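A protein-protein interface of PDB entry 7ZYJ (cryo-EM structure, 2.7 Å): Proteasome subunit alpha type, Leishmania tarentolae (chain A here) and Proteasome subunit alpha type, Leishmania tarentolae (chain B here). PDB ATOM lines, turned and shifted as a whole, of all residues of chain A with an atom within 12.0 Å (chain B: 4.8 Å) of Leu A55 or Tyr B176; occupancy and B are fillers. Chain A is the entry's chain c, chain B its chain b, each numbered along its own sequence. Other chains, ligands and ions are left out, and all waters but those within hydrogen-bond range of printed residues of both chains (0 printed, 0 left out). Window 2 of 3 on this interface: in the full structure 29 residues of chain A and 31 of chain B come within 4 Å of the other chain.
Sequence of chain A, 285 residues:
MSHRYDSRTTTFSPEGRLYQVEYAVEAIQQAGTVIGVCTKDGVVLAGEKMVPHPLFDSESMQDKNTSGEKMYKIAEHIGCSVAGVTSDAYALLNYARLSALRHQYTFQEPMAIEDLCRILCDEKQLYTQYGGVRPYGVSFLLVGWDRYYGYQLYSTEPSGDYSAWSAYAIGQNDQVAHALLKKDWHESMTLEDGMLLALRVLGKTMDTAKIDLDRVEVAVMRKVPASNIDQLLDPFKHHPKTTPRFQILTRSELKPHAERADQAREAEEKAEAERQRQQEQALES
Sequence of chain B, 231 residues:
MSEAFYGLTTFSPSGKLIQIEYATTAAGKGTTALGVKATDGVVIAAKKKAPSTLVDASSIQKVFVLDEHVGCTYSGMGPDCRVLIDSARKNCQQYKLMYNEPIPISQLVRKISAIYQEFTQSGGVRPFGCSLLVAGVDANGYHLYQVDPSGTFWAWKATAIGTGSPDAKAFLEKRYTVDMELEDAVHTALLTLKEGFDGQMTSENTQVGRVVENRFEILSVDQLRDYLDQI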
ATOM      1  N   LYS A  49      28.716   7.137   8.383  1.00  0.00           N
ATOM      2  CA  LYS A  49      27.966   7.180   9.626  1.00  0.00           C
ATOM      3  C   LYS A  49      28.821   7.809  10.719  1.00  0.00           C
ATOM      4  O   LYS A  49      30.051   7.843  10.635  1.00  0.00           O
ATOM      5  CB  LYS A  49      27.504   5.777  10.031  1.00  0.00           C
ATOM      6  CG  LYS A  49      28.618   4.770  10.251  1.00  0.00           C
ATOM      7  CD  LYS A  49      28.040   3.386  10.504  1.00  0.00           C
ATOM      8  CE  LYS A  49      29.127   2.360  10.767  1.00  0.00           C
ATOM      9  NZ  LYS A  49      29.823   2.621  12.055  1.00  0.00           N
ATOM     10  N   MET A  50      28.149   8.323  11.746  1.00  0.00           N
ATOM     11  CA  MET A  50      28.831   9.064  12.795  1.00  0.00           C
ATOM     12  C   MET A  50      29.838   8.163  13.512  1.00  0.00           C
ATOM     13  O   MET A  50      29.701   6.935  13.551  1.00  0.00           O
ATOM     14  CB  MET A  50      27.814   9.645  13.778  1.00  0.00           C
ATOM     15  CG  MET A  50      28.405  10.573  14.828  1.00  0.00           C
ATOM     16  SD  MET A  50      29.076  12.083  14.102  1.00  0.00           S
ATOM     17  CE  MET A  50      30.263  12.564  15.353  1.00  0.00           C
ATOM     18  N   VAL A  51      30.873   8.791  14.064  1.00  0.00           N
ATOM     19  CA  VAL A  51      31.964   8.045  14.704  1.00  0.00           C
ATOM     20  C   VAL A  51      31.395   7.173  15.816  1.00  0.00           C
ATOM     21  O   VAL A  51      30.663   7.680  16.689  1.00  0.00           O
ATOM     22  CB  VAL A  51      33.026   9.011  15.253  1.00  0.00           C
ATOM     23  CG1 VAL A  51      34.153   8.240  15.922  1.00  0.00           C
ATOM     24  CG2 VAL A  51      33.563   9.898  14.141  1.00  0.00           C
ATOM     25  N   PRO A  52      31.686   5.873  15.839  1.00  0.00           N
ATOM     26  CA  PRO A  52      31.057   4.987  16.829  1.00  0.00           C
ATOM     27  C   PRO A  52      31.653   5.195  18.213  1.00  0.00           C
ATOM     28  O   PRO A  52      32.832   4.925  18.447  1.00  0.00           O
ATOM     29  CB  PRO A  52      31.354   3.584  16.288  1.00  0.00           C
ATOM     30  CG  PRO A  52      32.592   3.751  15.479  1.00  0.00           C
ATOM     31  CD  PRO A  52      32.543   5.135  14.894  1.00  0.00           C
ATOM     32  N   HIS A  53      30.823   5.684  19.128  1.00  0.00           N
ATOM     33  CA  HIS A  53      31.200   5.767  20.527  1.00  0.00           C
ATOM     34  C   HIS A  53      31.346   4.354  21.095  1.00  0.00           C
ATOM     35  O   HIS A  53      30.583   3.454  20.738  1.00  0.00           O
ATOM     36  CB  HIS A  53      30.144   6.558  21.297  1.00  0.00           C
ATOM     37  CG  HIS A  53      30.520   6.883  22.709  1.00  0.00           C
ATOM     38  ND1 HIS A  53      30.610   5.928  23.698  1.00  0.00           N
ATOM     39  CD2 HIS A  53      30.816   8.065  23.301  1.00  0.00           C
ATOM     40  CE1 HIS A  53      30.953   6.505  24.836  1.00  0.00           C
ATOM     41  NE2 HIS A  53      31.085   7.802  24.622  1.00  0.00           N
ATOM     42  N   PRO A  54      32.325   4.132  21.975  1.00  0.00           N
ATOM     43  CA  PRO A  54      32.535   2.772  22.506  1.00  0.00           C
ATOM     44  C   PRO A  54      31.354   2.222  23.284  1.00  0.00           C
ATOM     45  O   PRO A  54      31.291   1.007  23.500  1.00  0.00           O
ATOM     46  CB  PRO A  54      33.774   2.928  23.400  1.00  0.00           C
ATOM     47  CG  PRO A  54      33.912   4.397  23.636  1.00  0.00           C
ATOM     48  CD  PRO A  54      33.382   5.059  22.409  1.00  0.00           C
ATOM     49  N   LEU A  55      30.419   3.066  23.716  1.00  0.00           N
ATOM     50  CA  LEU A  55      29.258   2.617  24.468  1.00  0.00           C
ATOM     51  C   LEU A  55      28.015   2.429  23.605  1.00  0.00           C
ATOM     52  O   LEU A  55      26.963   2.069  24.140  1.00  0.00           O
ATOM     53  CB  LEU A  55      28.953   3.597  25.605  1.00  0.00           C
ATOM     54  CG  LEU A  55      29.923   3.551  26.787  1.00  0.00           C
ATOM     55  CD1 LEU A  55      29.694   4.728  27.722  1.00  0.00           C
ATOM     56  CD2 LEU A  55      29.801   2.232  27.534  1.00  0.00           C
ATOM     57  N   PHE A  56      28.104   2.668  22.297  1.00  0.00           N
ATOM     58  CA  PHE A  56      26.997   2.320  21.415  1.00  0.00           C
ATOM     59  C   PHE A  56      26.746   0.820  21.436  1.00  0.00           C
ATOM     60  O   PHE A  56      27.679   0.014  21.480  1.00  0.00           O
ATOM     61  CB  PHE A  56      27.268   2.770  19.976  1.00  0.00           C
ATOM     62  CG  PHE A  56      27.267   4.259  19.782  1.00  0.00           C
ATOM     63  CD1 PHE A  56      26.749   5.103  20.746  1.00  0.00           C
ATOM     64  CD2 PHE A  56      27.753   4.809  18.608  1.00  0.00           C
ATOM     65  CE1 PHE A  56      26.737   6.471  20.551  1.00  0.00           C
ATOM     66  CE2 PHE A  56      27.743   6.174  18.409  1.00  0.00           C
ATOM     67  CZ  PHE A  56      27.236   7.007  19.382  1.00  0.00           C
ATOM     68  N   ASP A  57      25.472   0.449  21.400  1.00  0.00           N
ATOM     69  CA  ASP A  57      25.063  -0.938  21.284  1.00  0.00           C
ATOM     70  C   ASP A  57      24.286  -1.122  19.990  1.00  0.00           C
ATOM     71  O   ASP A  57      23.599  -0.209  19.523  1.00  0.00           O
ATOM     72  CB  ASP A  57      24.201  -1.373  22.473  1.00  0.00           C
ATOM     73  CG  ASP A  57      24.158  -2.878  22.638  1.00  0.00           C
ATOM     74  OD1 ASP A  57      24.995  -3.570  22.019  1.00  0.00           O
ATOM     75  OD2 ASP A  57      23.288  -3.371  23.384  1.00  0.00           O
ATOM     76  N   SER A  58      24.410  -2.307  19.408  1.00  0.00           N
ATOM     77  CA  SER A  58      23.691  -2.652  18.191  1.00  0.00           C
ATOM     78  C   SER A  58      22.366  -3.297  18.565  1.00  0.00           C
ATOM     79  O   SER A  58      22.331  -4.234  19.369  1.00  0.00           O
ATOM     80  CB  SER A  58      24.514  -3.598  17.317  1.00  0.00           C
ATOM     81  OG  SER A  58      24.649  -4.870  17.925  1.00  0.00           O
ATOM     82  N   GLU A  59      21.279  -2.785  17.992  1.00  0.00           N
ATOM     83  CA  GLU A  59      19.974  -3.403  18.173  1.00  0.00           C
ATOM     84  C   GLU A  59      20.016  -4.804  17.584  1.00  0.00           C
ATOM     85  O   GLU A  59      20.183  -4.963  16.370  1.00  0.00           O
ATOM     86  CB  GLU A  59      18.883  -2.563  17.509  1.00  0.00           C
ATOM     87  CG  GLU A  59      18.924  -1.095  17.890  1.00  0.00           C
ATOM     88  CD  GLU A  59      17.927  -0.262  17.112  1.00  0.00           C
ATOM     89  OE1 GLU A  59      17.253  -0.817  16.222  1.00  0.00           O
ATOM     90  OE2 GLU A  59      17.825   0.952  17.384  1.00  0.00           O
ATOM     91  N   SER A  60      19.871  -5.826  18.424  1.00  0.00           N
ATOM     92  CA  SER A  60      20.060  -7.194  17.960  1.00  0.00           C
ATOM     93  C   SER A  60      18.879  -7.630  17.106  1.00  0.00           C
ATOM     94  O   SER A  60      18.153  -8.564  17.459  1.00  0.00           O
ATOM     95  CB  SER A  60      20.244  -8.143  19.146  1.00  0.00           C
ATOM     96  OG  SER A  60      21.431  -7.841  19.859  1.00  0.00           O
ATOM     97  N   GLU A  69      22.138   2.104  10.016  1.00  0.00           N
ATOM     98  CA  GLU A  69      22.284   3.407  10.651  1.00  0.00           C
ATOM     99  C   GLU A  69      22.047   4.555   9.677  1.00  0.00           C
ATOM    100  O   GLU A  69      21.771   5.677  10.118  1.00  0.00           O
ATOM    101  CB  GLU A  69      23.673   3.533  11.280  1.00  0.00           C
ATOM    102  CG  GLU A  69      23.801   4.668  12.285  1.00  0.00           C
ATOM    103  CD  GLU A  69      25.210   4.823  12.818  1.00  0.00           C
ATOM    104  OE1 GLU A  69      25.757   3.836  13.354  1.00  0.00           O
ATOM    105  OE2 GLU A  69      25.768   5.935  12.709  1.00  0.00           O
ATOM    106  N   ASP A 214      34.681   1.417  10.549  1.00  0.00           N
ATOM    107  CA  ASP A 214      33.701   1.702  11.589  1.00  0.00           C
ATOM    108  C   ASP A 214      32.881   2.952  11.309  1.00  0.00           C
ATOM    109  O   ASP A 214      32.022   3.303  12.125  1.00  0.00           O
ATOM    110  CB  ASP A 214      34.400   1.851  12.944  1.00  0.00           C
ATOM    111  CG  ASP A 214      34.947   0.536  13.468  1.00  0.00           C
ATOM    112  OD1 ASP A 214      34.835  -0.486  12.759  1.00  0.00           O
ATOM    113  OD2 ASP A 214      35.488   0.524  14.595  1.00  0.00           O
ATOM    114  N   VAL B  36      22.332   0.972  32.594  1.00  0.00           N
ATOM    115  CA  VAL B  36      23.453   0.077  32.335  1.00  0.00           C
ATOM    116  C   VAL B  36      22.909  -1.254  31.839  1.00  0.00           C
ATOM    117  O   VAL B  36      22.042  -1.855  32.484  1.00  0.00           O
ATOM    118  CB  VAL B  36      24.323  -0.139  33.589  1.00  0.00           C
ATOM    119  CG1 VAL B  36      25.520  -1.014  33.258  1.00  0.00           C
ATOM    120  CG2 VAL B  36      24.772   1.190  34.171  1.00  0.00           C
ATOM    121  N   LYS B  37      23.421  -1.714  30.703  1.00  0.00           N
ATOM    122  CA  LYS B  37      23.086  -3.023  30.166  1.00  0.00           C
ATOM    123  C   LYS B  37      24.111  -4.057  30.628  1.00  0.00           C
ATOM    124  O   LYS B  37      25.260  -3.734  30.936  1.00  0.00           O
ATOM    125  CB  LYS B  37      23.025  -2.970  28.637  1.00  0.00           C
ATOM    126  CG  LYS B  37      22.592  -4.261  27.963  1.00  0.00           C
ATOM    127  CD  LYS B  37      22.509  -4.098  26.459  1.00  0.00           C
ATOM    128  CE  LYS B  37      22.140  -5.407  25.787  1.00  0.00           C
ATOM    129  NZ  LYS B  37      22.036  -5.263  24.310  1.00  0.00           N
ATOM    130  N   ALA B 155      20.756   3.080  20.667  1.00  0.00           N
ATOM    131  CA  ALA B 155      20.845   1.893  21.508  1.00  0.00           C
ATOM    132  C   ALA B 155      22.167   1.953  22.263  1.00  0.00           C
ATOM    133  O   ALA B 155      23.232   2.102  21.654  1.00  0.00           O
ATOM    134  CB  ALA B 155      20.732   0.621  20.673  1.00  0.00           C
ATOM    135  N   TRP B 156      22.102   1.847  23.583  1.00  0.00           N
ATOM    136  CA  TRP B 156      23.256   2.041  24.444  1.00  0.00           C
ATOM    137  C   TRP B 156      23.580   0.776  25.227  1.00  0.00           C
ATOM    138  O   TRP B 156      22.720  -0.069  25.482  1.00  0.00           O
ATOM    139  CB  TRP B 156      23.008   3.194  25.421  1.00  0.00           C
ATOM    140  CG  TRP B 156      23.036   4.548  24.795  1.00  0.00           C
ATOM    141  CD1 TRP B 156      21.962   5.298  24.421  1.00  0.00           C
ATOM    142  CD2 TRP B 156      24.195   5.334  24.500  1.00  0.00           C
ATOM    143  NE1 TRP B 156      22.380   6.496  23.895  1.00  0.00           N
ATOM    144  CE2 TRP B 156      23.747   6.543  23.935  1.00  0.00           C
ATOM    145  CE3 TRP B 156      25.569   5.130  24.655  1.00  0.00           C
ATOM    146  CZ2 TRP B 156      24.623   7.544  23.523  1.00  0.00           C
ATOM    147  CZ3 TRP B 156      26.437   6.123  24.245  1.00  0.00           C
ATOM    148  CH2 TRP B 156      25.961   7.316  23.688  1.00  0.00           C
ATOM    149  N   LYS B 157      24.853   0.657  25.603  1.00  0.00           N
ATOM    150  CA  LYS B 157      25.282  -0.318  26.595  1.00  0.00           C
ATOM    151  C   LYS B 157      25.314   0.261  28.000  1.00  0.00           C
ATOM    152  O   LYS B 157      25.042  -0.461  28.965  1.00  0.00           O
ATOM    153  CB  LYS B 157      26.670  -0.863  26.243  1.00  0.00           C
ATOM    154  CG  LYS B 157      26.682  -1.831  25.075  1.00  0.00           C
ATOM    155  CD  LYS B 157      28.084  -2.345  24.801  1.00  0.00           C
ATOM    156  CE  LYS B 157      28.946  -1.267  24.168  1.00  0.00           C
ATOM    157  NZ  LYS B 157      30.253  -1.798  23.697  1.00  0.00           N
ATOM    158  N   ALA B 158      25.639   1.545  28.126  1.00  0.00           N
ATOM    159  CA  ALA B 158      25.596   2.251  29.404  1.00  0.00           C
ATOM    160  C   ALA B 158      25.598   3.738  29.099  1.00  0.00           C
ATOM    161  O   ALA B 158      26.490   4.220  28.394  1.00  0.00           O
ATOM    162  CB  ALA B 158      26.782   1.873  30.290  1.00  0.00           C
ATOM    163  N   LYS B 169      28.771   9.579  32.274  1.00  0.00           N
ATOM    164  CA  LYS B 169      29.153   8.765  31.125  1.00  0.00           C
ATOM    165  C   LYS B 169      30.646   8.461  31.132  1.00  0.00           C
ATOM    166  O   LYS B 169      31.057   7.340  30.809  1.00  0.00           O
ATOM    167  CB  LYS B 169      28.749   9.464  29.827  1.00  0.00           C
ATOM    168  CG  LYS B 169      27.248   9.511  29.592  1.00  0.00           C
ATOM    169  CD  LYS B 169      26.900  10.350  28.374  1.00  0.00           C
ATOM    170  CE  LYS B 169      27.303   9.655  27.086  1.00  0.00           C
ATOM    171  NZ  LYS B 169      26.856  10.414  25.885  1.00  0.00           N
ATOM    172  N   LEU B 172      31.159   5.792  33.727  1.00  0.00           N
ATOM    173  CA  LEU B 172      30.684   4.497  33.254  1.00  0.00           C
ATOM    174  C   LEU B 172      31.600   3.912  32.188  1.00  0.00           C
ATOM    175  O   LEU B 172      31.711   2.687  32.074  1.00  0.00           O
ATOM    176  CB  LEU B 172      29.262   4.625  32.710  1.00  0.00           C
ATOM    177  CG  LEU B 172      28.131   4.622  33.737  1.00  0.00           C
ATOM    178  CD1 LEU B 172      26.893   5.303  33.173  1.00  0.00           C
ATOM    179  CD2 LEU B 172      27.816   3.203  34.179  1.00  0.00           C
ATOM    180  N   GLU B 173      32.254   4.767  31.398  1.00  0.00           N
ATOM    181  CA  GLU B 173      33.095   4.283  30.309  1.00  0.00           C
ATOM    182  C   GLU B 173      34.252   3.438  30.826  1.00  0.00           C
ATOM    183  O   GLU B 173      34.568   2.390  30.251  1.00  0.00           O
ATOM    184  CB  GLU B 173      33.618   5.466  29.494  1.00  0.00           C
ATOM    185  CG  GLU B 173      33.906   5.152  28.037  1.00  0.00           C
ATOM    186  CD  GLU B 173      34.592   6.302  27.325  1.00  0.00           C
ATOM    187  OE1 GLU B 173      34.970   7.279  28.005  1.00  0.00           O
ATOM    188  OE2 GLU B 173      34.754   6.231  26.090  1.00  0.00           O
ATOM    189  N   LYS B 174      34.896   3.871  31.912  1.00  0.00           N
ATOM    190  CA  LYS B 174      36.047   3.137  32.425  1.00  0.00           C
ATOM    191  C   LYS B 174      35.643   1.876  33.180  1.00  0.00           C
ATOM    192  O   LYS B 174      36.412   0.910  33.213  1.00  0.00           O
ATOM    193  CB  LYS B 174      36.895   4.038  33.324  1.00  0.00           C
ATOM    194  CG  LYS B 174      36.219   4.462  34.616  1.00  0.00           C
ATOM    195  CD  LYS B 174      37.110   5.392  35.422  1.00  0.00           C
ATOM    196  CE  LYS B 174      38.314   4.653  35.984  1.00  0.00           C
ATOM    197  NZ  LYS B 174      37.922   3.634  36.997  1.00  0.00           N
ATOM    198  N   ARG B 175      34.455   1.859  33.788  1.00  0.00           N
ATOM    199  CA  ARG B 175      34.055   0.717  34.601  1.00  0.00           C
ATOM    200  C   ARG B 175      33.262  -0.327  33.827  1.00  0.00           C
ATOM    201  O   ARG B 175      33.199  -1.480  34.269  1.00  0.00           O
ATOM    202  CB  ARG B 175      33.235   1.182  35.807  1.00  0.00           C
ATOM    203  CG  ARG B 175      33.931   2.220  36.668  1.00  0.00           C
ATOM    204  CD  ARG B 175      33.340   2.260  38.067  1.00  0.00           C
ATOM    205  NE  ARG B 175      33.895   1.226  38.933  1.00  0.00           N
ATOM    206  CZ  ARG B 175      33.299   0.073  39.205  1.00  0.00           C
ATOM    207  NH1 ARG B 175      32.116  -0.230  38.696  1.00  0.00           N
ATOM    208  NH2 ARG B 175      33.904  -0.797  40.009  1.00  0.00           N
ATOM    209  N   TYR B 176      32.656   0.036  32.700  1.00  0.00           N
ATOM    210  CA  TYR B 176      31.839  -0.913  31.957  1.00  0.00           C
ATOM    211  C   TYR B 176      32.703  -2.004  31.338  1.00  0.00           C
ATOM    212  O   TYR B 176      33.806  -1.744  30.847  1.00  0.00           O
ATOM    213  CB  TYR B 176      31.035  -0.206  30.866  1.00  0.00           C
ATOM    214  CG  TYR B 176      30.099  -1.138  30.129  1.00  0.00           C
ATOM    215  CD1 TYR B 176      28.985  -1.673  30.762  1.00  0.00           C
ATOM    216  CD2 TYR B 176      30.333  -1.490  28.808  1.00  0.00           C
ATOM    217  CE1 TYR B 176      28.129  -2.530  30.099  1.00  0.00           C
ATOM    218  CE2 TYR B 176      29.481  -2.346  28.135  1.00  0.00           C
ATOM    219  CZ  TYR B 176      28.380  -2.862  28.786  1.00  0.00           C
ATOM    220  OH  TYR B 176      27.529  -3.715  28.123  1.00  0.00           O
ATOM    221  N   THR B 177      32.188  -3.231  31.364  1.00  0.00           N
ATOM    222  CA  THR B 177      32.875  -4.390  30.816  1.00  0.00           C
ATOM    223  C   THR B 177      31.889  -5.157  29.948  1.00  0.00           C
ATOM    224  O   THR B 177      30.703  -5.235  30.279  1.00  0.00           O
ATOM    225  CB  THR B 177      33.428  -5.286  31.931  1.00  0.00           C
ATOM    226  OG1 THR B 177      34.241  -4.500  32.811  1.00  0.00           O
ATOM    227  CG2 THR B 177      34.281  -6.399  31.350  1.00  0.00           C
ATOM    228  N   VAL B 178      32.379  -5.717  28.838  1.00  0.00           N
ATOM    229  CA  VAL B 178      31.500  -6.347  27.859  1.00  0.00           C
ATOM    230  C   VAL B 178      30.734  -7.526  28.449  1.00  0.00           C
ATOM    231  O   VAL B 178      29.597  -7.786  28.043  1.00  0.00           O
ATOM    232  CB  VAL B 178      32.311  -6.770  26.612  1.00  0.00           C
ATOM    233  CG1 VAL B 178      33.326  -7.853  26.957  1.00  0.00           C
ATOM    234  CG2 VAL B 178      31.383  -7.226  25.493  1.00  0.00           C
ATOM    235  N   MET B 180      29.818  -7.974  31.737  1.00  0.00           N
ATOM    236  CA  MET B 180      29.298  -7.672  33.063  1.00  0.00           C
ATOM    237  C   MET B 180      27.969  -8.383  33.285  1.00  0.00           C
ATOM    238  O   MET B 180      27.150  -8.501  32.370  1.00  0.00           O
ATOM    239  CB  MET B 180      29.119  -6.166  33.251  1.00  0.00           C
ATOM    240  CG  MET B 180      28.791  -5.775  34.686  1.00  0.00           C
ATOM    241  SD  MET B 180      28.838  -4.004  35.028  1.00  0.00           S
ATOM    242  CE  MET B 180      29.943  -3.435  33.749  1.00  0.00           C
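Along chain B the printed residues that touch a printed residue of chain A span positions 37 to 176.
Of the 14 printed residues of chain A, 5 touch a printed residue of chain B.
Printed residues of chain A that touch a printed residue of chain B: Pro A54, Leu A55, Phe A56, Asp A57 and Glu A59.
Hydrophobic or aromatic side chains of chain A within 4 Å of the printed part of chain B: Pro A54, Leu A55 and Phe A56.
Among the printed residues, 14 pairs touch across the chains.
Among the printed residues, Asp or Glu carboxylates within 4 Å of a Lys or Arg side-chain nitrogen of the other chain: Asp A57 with Lys B37 (2.5 Å).
The side-chain amino group (NZ) of Lys B37 is in salt-bridge range of the side-chain carboxylate (OD2) of Asp A57 (2.5 Å).
The backbone carbonyl oxygen of Ala B155 lies within hydrogen-bond range of the backbone NH of Asp A57, 2.8 Å away.
The side-chain amino group (NZ) of Lys B157 sits at hydrogen-bond distance from the backbone carbonyl oxygen (O) of Pro A54, at 3.0 Å.
The backbone NH (N) of Lys B157 lies within hydrogen-bond range of the backbone carbonyl oxygen (O) of Leu A55 (2.9 Å).
Among the printed residues, pairs that only touch across the chains: Pro A54 with Glu B173, Leu A55 with Trp B156, Leu A55 with Ala B158, Leu A55 with Tyr B176, Phe A56 with Ala B155, Phe A56 with Trp B156, Phe A56 with Lys B157, Asp A57 with Trp B156, Asp A57 with Lys B157 and Glu A59 with Ala B155.
Leu A55 touches just these residues of chain B: Trp B156 (3.4 Å), Lys B157 (2.9 Å), Ala B158 (3.3 Å) and Tyr B176 (3.97 Å).
Tyr B176 touches one residue of chain A.
No residue of chain A comes within 4 Å of Val B36.
Of chain A, only Phe A56 (3.7 Å), Asp A57 (2.8 Å) and Glu A59 (3.7 Å) come within 4 Å of Ala B155.
Trp B156 touches three residues of chain A.
Printed residues of chain A within 4 Å of Ala B158: Leu A55 (3.3 Å).
Lys B169 touches none of the printed residues of chain A.
No residue of chain A comes within 4 Å of Leu B172.
No residue of chain A comes within 4 Å of Val B178.
No residue of chain A comes within 4 Å of Met B180.
Printed residues of chain B within 4 Å of Phe A56: Ala B155, Trp B156 and Lys B157.
Of the printed residues of chain B, Glu A59 touches Ala B155 (3.7 Å).
Of the printed residues of chain A, Glu B173 touches Pro A54 (3.2 Å).
Ser A60 touches none of the printed residues of chain B.
The backbone NH (N) of Lys B37 lies within hydrogen-bond range of the backbone carbonyl oxygen (O) of Lys B157 (2.7 Å).
A ring nitrogen (ND1) of His A53 sits at hydrogen-bond distance from the backbone NH (N) of Leu A55 (2.9 Å).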
